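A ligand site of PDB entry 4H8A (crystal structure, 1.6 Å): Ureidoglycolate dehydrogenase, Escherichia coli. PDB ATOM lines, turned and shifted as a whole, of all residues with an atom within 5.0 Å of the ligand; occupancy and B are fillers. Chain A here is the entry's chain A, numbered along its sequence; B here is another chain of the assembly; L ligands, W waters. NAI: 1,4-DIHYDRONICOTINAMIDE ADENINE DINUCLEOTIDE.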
ATOM      1  N   ILE A  43      -6.199  13.496 -32.791  1.00  0.00           N
ATOM      2  CA  ILE A  43      -4.951  13.686 -32.046  1.00  0.00           C
ATOM      3  C   ILE A  43      -3.877  12.816 -32.702  1.00  0.00           C
ATOM      4  O   ILE A  43      -3.362  11.864 -32.095  1.00  0.00           O
ATOM      5  CB  ILE A  43      -5.129  13.311 -30.561  1.00  0.00           C
ATOM      6  CG1 ILE A  43      -6.450  13.882 -30.038  1.00  0.00           C
ATOM      7  CG2 ILE A  43      -3.940  13.814 -29.741  1.00  0.00           C
ATOM      8  CD1 ILE A  43      -6.872  13.355 -28.659  1.00  0.00           C
ATOM      9  N   HIS A  46      -0.368  11.440 -31.446  1.00  0.00           N
ATOM     10  CA  HIS A  46      -0.323  10.342 -30.502  1.00  0.00           C
ATOM     11  C   HIS A  46      -1.060   9.141 -31.025  1.00  0.00           C
ATOM     12  O   HIS A  46      -1.490   8.263 -30.252  1.00  0.00           O
ATOM     13  CB  HIS A  46      -0.852  10.782 -29.145  1.00  0.00           C
ATOM     14  CG  HIS A  46       0.014  11.809 -28.466  1.00  0.00           C
ATOM     15  ND1 HIS A  46      -0.230  13.125 -28.571  1.00  0.00           N
ATOM     16  CD2 HIS A  46       1.157  11.679 -27.691  1.00  0.00           C
ATOM     17  CE1 HIS A  46       0.705  13.810 -27.877  1.00  0.00           C
ATOM     18  NE2 HIS A  46       1.560  12.920 -27.347  1.00  0.00           N
ATOM     19  N   HIS A 118       5.567   5.716 -22.780  1.00  0.00           N
ATOM     20  CA  HIS A 118       4.620   6.701 -23.296  1.00  0.00           C
ATOM     21  C   HIS A 118       3.189   6.130 -23.370  1.00  0.00           C
ATOM     22  O   HIS A 118       2.993   5.012 -23.879  1.00  0.00           O
ATOM     23  CB  HIS A 118       5.105   7.159 -24.674  1.00  0.00           C
ATOM     24  CG  HIS A 118       4.328   8.288 -25.252  1.00  0.00           C
ATOM     25  ND1 HIS A 118       3.413   8.109 -26.270  1.00  0.00           N
ATOM     26  CD2 HIS A 118       4.352   9.610 -24.993  1.00  0.00           C
ATOM     27  CE1 HIS A 118       2.894   9.278 -26.599  1.00  0.00           C
ATOM     28  NE2 HIS A 118       3.448  10.212 -25.835  1.00  0.00           N
ATOM     29  N   SER A 119       2.206   6.857 -22.843  1.00  0.00           N
ATOM     30  CA  SER A 119       0.827   6.341 -22.792  1.00  0.00           C
ATOM     31  C   SER A 119      -0.153   6.991 -23.770  1.00  0.00           C
ATOM     32  O   SER A 119      -1.340   6.622 -23.805  1.00  0.00           O
ATOM     33  CB  SER A 119       0.272   6.407 -21.367  1.00  0.00           C
ATOM     34  OG  SER A 119       0.205   7.740 -20.917  1.00  0.00           O
ATOM     35  N   GLY A 120       0.328   7.963 -24.550  1.00  0.00           N
ATOM     36  CA  GLY A 120      -0.452   8.520 -25.650  1.00  0.00           C
ATOM     37  C   GLY A 120      -1.440   9.611 -25.271  1.00  0.00           C
ATOM     38  O   GLY A 120      -1.171  10.441 -24.406  1.00  0.00           O
ATOM     39  N   ALA A 121      -2.582   9.622 -25.964  1.00  0.00           N
ATOM     40  CA  ALA A 121      -3.639  10.586 -25.726  1.00  0.00           C
ATOM     41  C   ALA A 121      -4.340  10.212 -24.423  1.00  0.00           C
ATOM     42  O   ALA A 121      -5.145   9.290 -24.395  1.00  0.00           O
ATOM     43  CB  ALA A 121      -4.626  10.567 -26.880  1.00  0.00           C
ATOM     44  N   ILE A 122      -4.026  10.919 -23.341  1.00  0.00           N
ATOM     45  CA  ILE A 122      -4.452  10.431 -22.041  1.00  0.00           C
ATOM     46  C   ILE A 122      -5.938  10.568 -21.740  1.00  0.00           C
ATOM     47  O   ILE A 122      -6.419  10.007 -20.744  1.00  0.00           O
ATOM     48  CB  ILE A 122      -3.595  10.997 -20.874  1.00  0.00           C
ATOM     49  CG1 ILE A 122      -3.715  12.519 -20.806  1.00  0.00           C
ATOM     50  CG2 ILE A 122      -2.131  10.541 -21.016  1.00  0.00           C
ATOM     51  CD1 ILE A 122      -3.266  13.089 -19.462  1.00  0.00           C
ATOM     52  N   SER A 123      -6.677  11.271 -22.593  1.00  0.00           N
ATOM     53  CA  SER A 123      -8.131  11.335 -22.408  1.00  0.00           C
ATOM     54  C   SER A 123      -8.768   9.968 -22.622  1.00  0.00           C
ATOM     55  O   SER A 123      -9.904   9.738 -22.200  1.00  0.00           O
ATOM     56  CB  SER A 123      -8.806  12.397 -23.272  1.00  0.00           C
ATOM     57  OG  SER A 123      -8.564  12.199 -24.660  1.00  0.00           O
ATOM     58  N   CYS A 140       0.166  13.254 -16.779  1.00  0.00           N
ATOM     59  CA  CYS A 140       1.420  12.497 -16.787  1.00  0.00           C
ATOM     60  C   CYS A 140       2.611  13.354 -17.136  1.00  0.00           C
ATOM     61  O   CYS A 140       2.473  14.445 -17.683  1.00  0.00           O
ATOM     62  CB  CYS A 140       1.348  11.276 -17.722  1.00  0.00           C
ATOM     63  SG  CYS A 140       1.330  11.643 -19.467  1.00  0.00           S
ATOM     64  N   GLN A 141       3.781  12.826 -16.793  1.00  0.00           N
ATOM     65  CA  GLN A 141       5.046  13.469 -17.151  1.00  0.00           C
ATOM     66  C   GLN A 141       5.340  13.252 -18.623  1.00  0.00           C
ATOM     67  O   GLN A 141       4.880  12.272 -19.219  1.00  0.00           O
ATOM     68  CB  GLN A 141       6.189  12.830 -16.369  1.00  0.00           C
ATOM     69  CG  GLN A 141       6.162  13.058 -14.896  1.00  0.00           C
ATOM     70  CD  GLN A 141       7.295  12.343 -14.215  1.00  0.00           C
ATOM     71  OE1 GLN A 141       7.477  11.129 -14.410  1.00  0.00           O
ATOM     72  NE2 GLN A 141       8.078  13.070 -13.433  1.00  0.00           N
ATOM     73  N   SER A 142       6.134  14.148 -19.204  1.00  0.00           N
ATOM     74  CA  SER A 142       6.581  13.970 -20.577  1.00  0.00           C
ATOM     75  C   SER A 142       8.027  14.449 -20.747  1.00  0.00           C
ATOM     76  O   SER A 142       8.561  15.122 -19.847  1.00  0.00           O
ATOM     77  CB  SER A 142       5.630  14.680 -21.543  1.00  0.00           C
ATOM     78  OG  SER A 142       5.975  14.435 -22.894  1.00  0.00           O
ATOM     79  N   THR A 158       5.633  18.483 -21.916  1.00  0.00           N
ATOM     80  CA  THR A 158       4.341  19.020 -22.352  1.00  0.00           C
ATOM     81  C   THR A 158       3.195  18.518 -21.471  1.00  0.00           C
ATOM     82  O   THR A 158       2.036  18.867 -21.714  1.00  0.00           O
ATOM     83  CB  THR A 158       4.052  18.667 -23.825  1.00  0.00           C
ATOM     84  OG1 THR A 158       4.230  17.262 -24.004  1.00  0.00           O
ATOM     85  CG2 THR A 158       5.030  19.429 -24.729  1.00  0.00           C
ATOM     86  N   ASN A 159       3.560  17.693 -20.500  1.00  0.00           N
ATOM     87  CA  ASN A 159       2.757  17.375 -19.303  1.00  0.00           C
ATOM     88  C   ASN A 159       1.257  17.650 -19.422  1.00  0.00           C
ATOM     89  O   ASN A 159       0.760  18.698 -19.025  1.00  0.00           O
ATOM     90  CB  ASN A 159       3.349  18.102 -18.082  1.00  0.00           C
ATOM     91  CG  ASN A 159       4.726  17.603 -17.726  1.00  0.00           C
ATOM     92  OD1 ASN A 159       5.404  16.975 -18.555  1.00  0.00           O
ATOM     93  ND2 ASN A 159       5.161  17.868 -16.515  1.00  0.00           N
ATOM     94  N   PRO A 160       0.528  16.669 -19.966  1.00  0.00           N
ATOM     95  CA  PRO A 160      -0.896  16.870 -20.247  1.00  0.00           C
ATOM     96  C   PRO A 160      -1.817  16.626 -19.054  1.00  0.00           C
ATOM     97  O   PRO A 160      -1.467  15.900 -18.112  1.00  0.00           O
ATOM     98  CB  PRO A 160      -1.177  15.795 -21.313  1.00  0.00           C
ATOM     99  CG  PRO A 160      -0.198  14.705 -20.986  1.00  0.00           C
ATOM    100  CD  PRO A 160       1.042  15.386 -20.484  1.00  0.00           C
ATOM    101  N   THR A 174     -15.486  15.435 -22.581  1.00  0.00           N
ATOM    102  CA  THR A 174     -14.057  15.096 -22.527  1.00  0.00           C
ATOM    103  C   THR A 174     -13.214  16.325 -22.840  1.00  0.00           C
ATOM    104  O   THR A 174     -13.461  17.010 -23.837  1.00  0.00           O
ATOM    105  CB  THR A 174     -13.703  14.013 -23.571  1.00  0.00           C
ATOM    106  OG1 THR A 174     -14.575  12.894 -23.420  1.00  0.00           O
ATOM    107  CG2 THR A 174     -12.266  13.548 -23.407  1.00  0.00           C
ATOM    108  N   PHE A 175     -12.239  16.604 -21.984  1.00  0.00           N
ATOM    109  CA  PHE A 175     -11.322  17.734 -22.160  1.00  0.00           C
ATOM    110  C   PHE A 175      -9.892  17.200 -21.986  1.00  0.00           C
ATOM    111  O   PHE A 175      -9.640  16.409 -21.076  1.00  0.00           O
ATOM    112  CB  PHE A 175     -11.658  18.851 -21.149  1.00  0.00           C
ATOM    113  CG  PHE A 175     -10.683  19.993 -21.144  1.00  0.00           C
ATOM    114  CD1 PHE A 175     -10.510  20.814 -22.264  1.00  0.00           C
ATOM    115  CD2 PHE A 175      -9.960  20.297 -19.996  1.00  0.00           C
ATOM    116  CE1 PHE A 175      -9.625  21.878 -22.239  1.00  0.00           C
ATOM    117  CE2 PHE A 175      -9.084  21.364 -19.954  1.00  0.00           C
ATOM    118  CZ  PHE A 175      -8.909  22.164 -21.079  1.00  0.00           C
ATOM    119  N   ASP A 176      -8.964  17.606 -22.860  1.00  0.00           N
ATOM    120  CA  ASP A 176      -7.625  17.002 -22.871  1.00  0.00           C
ATOM    121  C   ASP A 176      -6.613  17.998 -23.437  1.00  0.00           C
ATOM    122  O   ASP A 176      -6.678  18.315 -24.631  1.00  0.00           O
ATOM    123  CB  ASP A 176      -7.638  15.733 -23.746  1.00  0.00           C
ATOM    124  CG  ASP A 176      -6.389  14.850 -23.594  1.00  0.00           C
ATOM    125  OD1 ASP A 176      -5.444  15.232 -22.875  1.00  0.00           O
ATOM    126  OD2 ASP A 176      -6.355  13.749 -24.210  1.00  0.00           O
ATOM    127  N   MET A 177      -5.669  18.479 -22.617  1.00  0.00           N
ATOM    128  CA  MET A 177      -4.743  19.534 -23.067  1.00  0.00           C
ATOM    129  C   MET A 177      -3.279  19.293 -22.690  1.00  0.00           C
ATOM    130  O   MET A 177      -2.969  18.799 -21.602  1.00  0.00           O
ATOM    131  CB  MET A 177      -5.172  20.894 -22.513  1.00  0.00           C
ATOM    132  CG  MET A 177      -5.354  20.862 -20.991  1.00  0.00           C
ATOM    133  SD  MET A 177      -5.558  22.476 -20.215  1.00  0.00           S
ATOM    134  CE  MET A 177      -3.855  22.937 -19.931  1.00  0.00           C
ATOM    135  N   ALA A 178      -2.372  19.667 -23.591  1.00  0.00           N
ATOM    136  CA  ALA A 178      -0.973  19.828 -23.229  1.00  0.00           C
ATOM    137  C   ALA A 178      -0.877  21.123 -22.456  1.00  0.00           C
ATOM    138  O   ALA A 178      -1.699  22.034 -22.637  1.00  0.00           O
ATOM    139  CB  ALA A 178      -0.095  19.905 -24.486  1.00  0.00           C
ATOM    140  N   GLN A 182       1.326  25.076 -27.589  1.00  0.00           N
ATOM    141  CA  GLN A 182       0.978  24.117 -28.621  1.00  0.00           C
ATOM    142  C   GLN A 182       1.716  22.816 -28.318  1.00  0.00           C
ATOM    143  O   GLN A 182       2.790  22.840 -27.710  1.00  0.00           O
ATOM    144  CB  GLN A 182       1.426  24.674 -29.982  1.00  0.00           C
ATOM    145  CG  GLN A 182       0.412  24.502 -31.094  1.00  0.00           C
ATOM    146  CD  GLN A 182      -0.994  24.891 -30.685  1.00  0.00           C
ATOM    147  OE1 GLN A 182      -1.302  26.069 -30.486  1.00  0.00           O
ATOM    148  NE2 GLN A 182      -1.861  23.891 -30.557  1.00  0.00           N
ATOM    149  N   ALA A 183       1.146  21.687 -28.721  1.00  0.00           N
ATOM    150  CA  ALA A 183       1.840  20.403 -28.601  1.00  0.00           C
ATOM    151  C   ALA A 183       3.044  20.361 -29.530  1.00  0.00           C
ATOM    152  O   ALA A 183       3.087  21.095 -30.524  1.00  0.00           O
ATOM    153  CB  ALA A 183       0.885  19.253 -28.900  1.00  0.00           C
ATOM    154  N   LYS A 186       2.947  20.028 -33.487  1.00  0.00           N
ATOM    155  CA  LYS A 186       2.662  21.188 -34.345  1.00  0.00           C
ATOM    156  C   LYS A 186       3.952  21.816 -34.846  1.00  0.00           C
ATOM    157  O   LYS A 186       3.983  22.416 -35.919  1.00  0.00           O
ATOM    158  CB  LYS A 186       1.823  22.220 -33.589  1.00  0.00           C
ATOM    159  CG  LYS A 186       0.473  21.693 -33.138  1.00  0.00           C
ATOM    160  CD  LYS A 186      -0.592  21.890 -34.206  1.00  0.00           C
ATOM    161  CE  LYS A 186      -1.770  20.961 -33.982  1.00  0.00           C
ATOM    162  NZ  LYS A 186      -1.811  20.444 -32.582  1.00  0.00           N
ATOM    163  N   TYR A 305     -18.708  25.690 -29.378  1.00  0.00           N
ATOM    164  CA  TYR A 305     -18.640  24.280 -29.032  1.00  0.00           C
ATOM    165  C   TYR A 305     -18.535  24.163 -27.514  1.00  0.00           C
ATOM    166  O   TYR A 305     -17.945  25.022 -26.875  1.00  0.00           O
ATOM    167  CB  TYR A 305     -17.360  23.663 -29.611  1.00  0.00           C
ATOM    168  CG  TYR A 305     -17.429  23.346 -31.076  1.00  0.00           C
ATOM    169  CD1 TYR A 305     -16.296  23.416 -31.872  1.00  0.00           C
ATOM    170  CD2 TYR A 305     -18.626  22.962 -31.666  1.00  0.00           C
ATOM    171  CE1 TYR A 305     -16.341  23.113 -33.227  1.00  0.00           C
ATOM    172  CE2 TYR A 305     -18.692  22.662 -33.021  1.00  0.00           C
ATOM    173  CZ  TYR A 305     -17.540  22.744 -33.787  1.00  0.00           C
ATOM    174  OH  TYR A 305     -17.609  22.456 -35.135  1.00  0.00           O
ATOM    175  N   TYR A 306     -19.104  23.109 -26.927  1.00  0.00           N
ATOM    176  CA  TYR A 306     -18.745  22.821 -25.533  1.00  0.00           C
ATOM    177  C   TYR A 306     -17.314  22.236 -25.549  1.00  0.00           C
ATOM    178  O   TYR A 306     -16.853  21.763 -26.583  1.00  0.00           O
ATOM    179  CB  TYR A 306     -19.771  21.897 -24.842  1.00  0.00           C
ATOM    180  CG  TYR A 306     -19.960  20.534 -25.476  1.00  0.00           C
ATOM    181  CD1 TYR A 306     -19.042  19.513 -25.271  1.00  0.00           C
ATOM    182  CD2 TYR A 306     -21.075  20.250 -26.273  1.00  0.00           C
ATOM    183  CE1 TYR A 306     -19.189  18.281 -25.822  1.00  0.00           C
ATOM    184  CE2 TYR A 306     -21.229  18.993 -26.856  1.00  0.00           C
ATOM    185  CZ  TYR A 306     -20.279  18.014 -26.622  1.00  0.00           C
ATOM    186  OH  TYR A 306     -20.388  16.755 -27.184  1.00  0.00           O
ATOM    187  N   PRO A 307     -16.598  22.284 -24.407  1.00  0.00           N
ATOM    188  CA  PRO A 307     -15.197  21.797 -24.469  1.00  0.00           C
ATOM    189  C   PRO A 307     -15.064  20.367 -24.969  1.00  0.00           C
ATOM    190  O   PRO A 307     -15.768  19.473 -24.504  1.00  0.00           O
ATOM    191  CB  PRO A 307     -14.731  21.883 -23.014  1.00  0.00           C
ATOM    192  CG  PRO A 307     -15.564  22.970 -22.425  1.00  0.00           C
ATOM    193  CD  PRO A 307     -16.916  22.847 -23.088  1.00  0.00           C
ATOM    194  N   GLY A 308     -14.163  20.162 -25.928  1.00  0.00           N
ATOM    195  CA  GLY A 308     -13.934  18.828 -26.459  1.00  0.00           C
ATOM    196  C   GLY A 308     -14.876  18.460 -27.596  1.00  0.00           C
ATOM    197  O   GLY A 308     -14.704  17.414 -28.216  1.00  0.00           O
ATOM    198  N   GLN A 309     -15.868  19.316 -27.868  1.00  0.00           N
ATOM    199  CA  GLN A 309     -16.890  18.980 -28.859  1.00  0.00           C
ATOM    200  C   GLN A 309     -16.276  18.882 -30.249  1.00  0.00           C
ATOM    201  O   GLN A 309     -16.734  18.091 -31.065  1.00  0.00           O
ATOM    202  CB  GLN A 309     -18.043  19.989 -28.857  1.00  0.00           C
ATOM    203  CG  GLN A 309     -19.224  19.564 -29.757  1.00  0.00           C
ATOM    204  CD  GLN A 309     -20.403  20.496 -29.683  1.00  0.00           C
ATOM    205  OE1 GLN A 309     -20.343  21.557 -29.058  1.00  0.00           O
ATOM    206  NE2 GLN A 309     -21.510  20.105 -30.319  1.00  0.00           N
ATOM    207  N   ASP A 310     -15.230  19.650 -30.490  1.00  0.00           N
ATOM    208  CA  ASP A 310     -14.552  19.592 -31.779  1.00  0.00           C
ATOM    209  C   ASP A 310     -14.038  18.174 -32.055  1.00  0.00           C
ATOM    210  O   ASP A 310     -14.201  17.650 -33.160  1.00  0.00           O
ATOM    211  CB  ASP A 310     -13.423  20.629 -31.870  1.00  0.00           C
ATOM    212  CG  ASP A 310     -12.368  20.464 -30.802  1.00  0.00           C
ATOM    213  OD1 ASP A 310     -12.709  20.062 -29.671  1.00  0.00           O
ATOM    214  OD2 ASP A 310     -11.184  20.751 -31.089  1.00  0.00           O
ATOM    215  N   GLN A 311     -13.469  17.548 -31.029  1.00  0.00           N
ATOM    216  CA  GLN A 311     -12.984  16.189 -31.151  1.00  0.00           C
ATOM    217  C   GLN A 311     -14.099  15.155 -31.156  1.00  0.00           C
ATOM    218  O   GLN A 311     -13.973  14.111 -31.797  1.00  0.00           O
ATOM    219  CB  GLN A 311     -11.983  15.865 -30.029  1.00  0.00           C
ATOM    220  CG  GLN A 311     -10.778  16.779 -30.012  1.00  0.00           C
ATOM    221  CD  GLN A 311      -9.718  16.277 -29.072  1.00  0.00           C
ATOM    222  OE1 GLN A 311      -9.849  15.194 -28.474  1.00  0.00           O
ATOM    223  NE2 GLN A 311      -8.651  17.044 -28.920  1.00  0.00           N
ATOM    224  N   PHE B 149     -15.087  30.079 -25.241  1.00  0.00           N
ATOM    225  CA  PHE B 149     -14.262  30.306 -26.420  1.00  0.00           C
ATOM    226  C   PHE B 149     -15.121  30.349 -27.673  1.00  0.00           C
ATOM    227  O   PHE B 149     -15.847  29.386 -27.971  1.00  0.00           O
ATOM    228  CB  PHE B 149     -13.191  29.224 -26.558  1.00  0.00           C
ATOM    229  CG  PHE B 149     -12.256  29.473 -27.712  1.00  0.00           C
ATOM    230  CD1 PHE B 149     -11.367  30.538 -27.674  1.00  0.00           C
ATOM    231  CD2 PHE B 149     -12.285  28.665 -28.839  1.00  0.00           C
ATOM    232  CE1 PHE B 149     -10.503  30.791 -28.726  1.00  0.00           C
ATOM    233  CE2 PHE B 149     -11.413  28.914 -29.909  1.00  0.00           C
ATOM    234  CZ  PHE B 149     -10.524  29.973 -29.848  1.00  0.00           C
ATOM    235  N   PRO B 225      -9.383  27.967 -25.682  1.00  0.00           N
ATOM    236  CA  PRO B 225     -10.158  26.778 -25.323  1.00  0.00           C
ATOM    237  C   PRO B 225      -9.646  26.108 -24.045  1.00  0.00           C
ATOM    238  O   PRO B 225     -10.414  25.393 -23.389  1.00  0.00           O
ATOM    239  CB  PRO B 225      -9.968  25.842 -26.522  1.00  0.00           C
ATOM    240  CG  PRO B 225      -9.484  26.747 -27.658  1.00  0.00           C
ATOM    241  CD  PRO B 225      -8.729  27.856 -26.994  1.00  0.00           C
ATOM    242  N   LYS B 226      -8.385  26.328 -23.672  1.00  0.00           N
ATOM    243  CA  LYS B 226      -7.840  25.638 -22.486  1.00  0.00           C
ATOM    244  C   LYS B 226      -8.368  26.205 -21.167  1.00  0.00           C
ATOM    245  O   LYS B 226      -8.770  25.447 -20.260  1.00  0.00           O
ATOM    246  CB  LYS B 226      -6.297  25.628 -22.527  1.00  0.00           C
ATOM    247  CG  LYS B 226      -5.761  24.727 -23.636  1.00  0.00           C
ATOM    248  CD  LYS B 226      -4.240  24.602 -23.641  1.00  0.00           C
ATOM    249  CE  LYS B 226      -3.794  23.862 -24.895  1.00  0.00           C
ATOM    250  NZ  LYS B 226      -2.319  23.657 -24.994  1.00  0.00           N
ATOM    251  N   TYR B 228     -11.085  27.768 -20.991  1.00  0.00           N
ATOM    252  CA  TYR B 228     -12.505  27.412 -21.117  1.00  0.00           C
ATOM    253  C   TYR B 228     -12.760  26.039 -20.516  1.00  0.00           C
ATOM    254  O   TYR B 228     -13.688  25.866 -19.714  1.00  0.00           O
ATOM    255  CB  TYR B 228     -12.852  27.460 -22.601  1.00  0.00           C
ATOM    256  CG  TYR B 228     -14.251  27.065 -23.025  1.00  0.00           C
ATOM    257  CD1 TYR B 228     -15.363  27.289 -22.227  1.00  0.00           C
ATOM    258  CD2 TYR B 228     -14.445  26.480 -24.278  1.00  0.00           C
ATOM    259  CE1 TYR B 228     -16.642  26.928 -22.668  1.00  0.00           C
ATOM    260  CE2 TYR B 228     -15.696  26.124 -24.730  1.00  0.00           C
ATOM    261  CZ  TYR B 228     -16.791  26.338 -23.921  1.00  0.00           C
ATOM    262  OH  TYR B 228     -18.029  25.976 -24.400  1.00  0.00           O
HETATM  263  PA  NAI L   1      -5.830  21.450 -28.270  1.00  0.00           P
HETATM  264  O1A NAI L   1      -6.199  21.226 -29.752  1.00  0.00           O
HETATM  265  O2A NAI L   1      -5.112  22.735 -28.068  1.00  0.00           O
HETATM  266  O5B NAI L   1      -7.215  21.530 -27.424  1.00  0.00           O
HETATM  267  C5B NAI L   1      -7.301  21.176 -26.058  1.00  0.00           C
HETATM  268  C4B NAI L   1      -8.648  20.868 -25.574  1.00  0.00           C
HETATM  269  O4B NAI L   1      -9.520  21.947 -25.893  1.00  0.00           O
HETATM  270  C3B NAI L   1      -9.201  19.673 -26.247  1.00  0.00           C
HETATM  271  O3B NAI L   1     -10.034  19.000 -25.315  1.00  0.00           O
HETATM  272  C2B NAI L   1      -9.977  20.194 -27.314  1.00  0.00           C
HETATM  273  O2B NAI L   1     -10.985  19.323 -27.687  1.00  0.00           O
HETATM  274  C1B NAI L   1     -10.506  21.494 -26.762  1.00  0.00           C
HETATM  275  N9A NAI L   1     -10.815  22.501 -27.767  1.00  0.00           N
HETATM  276  C8A NAI L   1      -9.936  23.024 -28.645  1.00  0.00           C
HETATM  277  N7A NAI L   1     -10.574  23.933 -29.414  1.00  0.00           N
HETATM  278  C5A NAI L   1     -11.865  24.002 -29.017  1.00  0.00           C
HETATM  279  C6A NAI L   1     -12.987  24.750 -29.419  1.00  0.00           C
HETATM  280  N6A NAI L   1     -12.917  25.688 -30.454  1.00  0.00           N
HETATM  281  N1A NAI L   1     -14.148  24.567 -28.782  1.00  0.00           N
HETATM  282  C2A NAI L   1     -14.256  23.690 -27.777  1.00  0.00           C
HETATM  283  N3A NAI L   1     -13.214  22.952 -27.371  1.00  0.00           N
HETATM  284  C4A NAI L   1     -12.008  23.095 -27.966  1.00  0.00           C
HETATM  285  O3  NAI L   1      -5.073  20.185 -27.797  1.00  0.00           O
HETATM  286  PN  NAI L   1      -3.582  19.940 -27.361  1.00  0.00           P
HETATM  287  O1N NAI L   1      -3.136  20.845 -26.214  1.00  0.00           O
HETATM  288  O2N NAI L   1      -2.610  20.118 -28.550  1.00  0.00           O
HETATM  289  O5D NAI L   1      -3.678  18.428 -26.937  1.00  0.00           O
HETATM  290  C5D NAI L   1      -2.607  17.547 -26.645  1.00  0.00           C
HETATM  291  C4D NAI L   1      -2.900  16.081 -26.843  1.00  0.00           C
HETATM  292  O4D NAI L   1      -1.700  15.403 -26.780  1.00  0.00           O
HETATM  293  C3D NAI L   1      -3.722  15.536 -25.741  1.00  0.00           C
HETATM  294  O3D NAI L   1      -4.499  14.414 -26.244  1.00  0.00           O
HETATM  295  C2D NAI L   1      -2.776  15.096 -24.813  1.00  0.00           C
HETATM  296  O2D NAI L   1      -3.265  14.021 -23.981  1.00  0.00           O
HETATM  297  C1D NAI L   1      -1.667  14.611 -25.648  1.00  0.00           C
HETATM  298  N1N NAI L   1      -0.337  14.675 -24.994  1.00  0.00           N
HETATM  299  C2N NAI L   1       0.248  13.558 -24.544  1.00  0.00           C
HETATM  300  C3N NAI L   1       1.504  13.632 -23.939  1.00  0.00           C
HETATM  301  C7N NAI L   1       2.152  12.444 -23.444  1.00  0.00           C
HETATM  302  O7N NAI L   1       1.517  11.423 -23.336  1.00  0.00           O
HETATM  303  N7N NAI L   1       3.585  12.471 -23.071  1.00  0.00           N
HETATM  304  C4N NAI L   1       2.123  14.886 -23.811  1.00  0.00           C
HETATM  305  C5N NAI L   1       1.473  16.026 -24.285  1.00  0.00           C
HETATM  306  C6N NAI L   1       0.224  15.891 -24.885  1.00  0.00           C
HETATM  307  O   HOH W   1     -15.927  26.803 -29.340  1.00  0.00           O
HETATM  308  O   HOH W   2      -2.011  22.985 -27.840  1.00  0.00           O
HETATM  309  O   HOH W   3     -10.604  22.933 -32.712  1.00  0.00           O
HETATM  310  O   HOH W   4      -6.496  16.855 -27.142  1.00  0.00           O
HETATM  311  O   HOH W   5      -4.691  20.691 -31.897  1.00  0.00           O
HETATM  312  O   HOH W   6      -8.547  19.742 -30.530  1.00  0.00           O
HETATM  313  O   HOH W   7      -6.422  24.925 -27.671  1.00  0.00           O
HETATM  314  O   HOH W   8     -11.159  16.549 -25.710  1.00  0.00           O
HETATM  315  O   HOH W   9      -7.465  22.799 -31.605  1.00  0.00           O
HETATM  316  O   HOH W  10      -2.526  18.076 -30.306  1.00  0.00           O
HETATM  317  O   HOH W  11       2.763   9.329 -21.505  1.00  0.00           O
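Water W5 lies within hydrogen-bond range of O1A of the ligand (2.7 Å) and NZ of Lys 186 (3.0 Å). Water W10 lies within hydrogen-bond range of an oxygen (O2N) of the ligand (2.7 Å) and the side-chain amino group of Lys 186 (3.4 Å). Water W6 lies within hydrogen-bond range of OD2 of Asp 310, O1A of the ligand and NE2 of Gln 311. Water W1 lies within hydrogen-bond range of N1A of the ligand (2.9 Å), O of Phe 149 of chain B (2.9 Å) and N of Tyr 305 (3.0 Å). Water W4 lies within hydrogen-bond range of NE2 of Gln 311 (2.8 Å), O of Asp 176 (2.9 Å) and O5D of the ligand (3.2 Å). Water W3 lies within hydrogen-bond range of OD2 of Asp 310 and N7A of the ligand.
N of Asp 176 sits at hydrogen-bond distance from O3B of the ligand. O of Asp 176 lies close to O3B of the ligand (3.5 Å). An oxygen (O2D) of the ligand is in hydrogen-bond range of the side-chain carboxylate (OD1) of Asp 176 (2.7 Å). The side-chain carboxylate (OD1) of Asp 310 lies within hydrogen-bond range of an oxygen (O2B) of the ligand (2.7 Å). An oxygen (O1N) of the ligand is in hydrogen-bond range of the backbone NH (N) of Ala 178, 3.0 Å away. ND1 of His 46 lies close to O4D of the ligand. N7N of the ligand sits at hydrogen-bond distance from OG of Ser 142 (3.1 Å). NZ of Lys 226 of chain B lies within salt-bridge range of O1N of the ligand, 3.2 Å away. N of Gly 308 lies within hydrogen-bond range of N3A of the ligand, at 3.3 Å. The backbone NH of Ile 122 is in hydrogen-bond range of an oxygen (O2D) of the ligand (3.3 Å). A ring nitrogen (NE2) of His 118 sits at hydrogen-bond distance from an oxygen (O7N) of the ligand (3.4 Å). O2B of the ligand lies close to NE2 of Gln 311 (3.5 Å).
The backbone carbonyl oxygen of Gly 120 sits close to an oxygen (O7N) of the ligand, 3.1 Å away. Merely in contact with the ligand: Ile 43 (3.5 Å), Ala 121 (3.9 Å), Cys 140 (3.9 Å), Thr 158 (3.0 Å), Pro 160 (3.5 Å), Phe 175 (3.6 Å), Met 177 (3.8 Å), Ala 183 (3.6 Å), Tyr 305 (3.4 Å), Tyr 306 (3.4 Å), Pro 307 (3.7 Å), Phe 149 of chain B (3.4 Å) and Pro 225 of chain B (3.5 Å). Hydrophobic or aromatic side chains that line the ligand: Ile 43, His 46, His 118, Ala 121, Ile 122, Pro 160, Phe 175, Ala 178, Ala 183, Tyr 305, Phe 149 of chain B and Pro 225 of chain B. Of the 33 residues printed, 24 come within 4 Å of the ligand. The nearest printed residue that does not touch the ligand is Gln 141 (4.1 Å).
The side-chain hydroxyl of Ser 123 sits at hydrogen-bond distance from the side-chain carboxylate of Asp 176, 2.7 Å away. NZ of Lys 226 of chain B is in hydrogen-bond range of O of Ala 178 (2.9 Å). The backbone NH (N) of Ser 142 lies within hydrogen-bond range of the side-chain amide oxygen (OD1) of Asn 159 (3.0 Å). The backbone carbonyl oxygen of Tyr 305 is in hydrogen-bond range of the side-chain hydroxyl of Tyr 228 of chain B (2.7 Å). The backbone NH (N) of Tyr 306 is in hydrogen-bond range of the side-chain amide oxygen (OE1) of Gln 309. The backbone carbonyl oxygen (O) of Pro 160 sits at hydrogen-bond distance from the backbone NH (N) of Cys 140 (3.4 Å).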
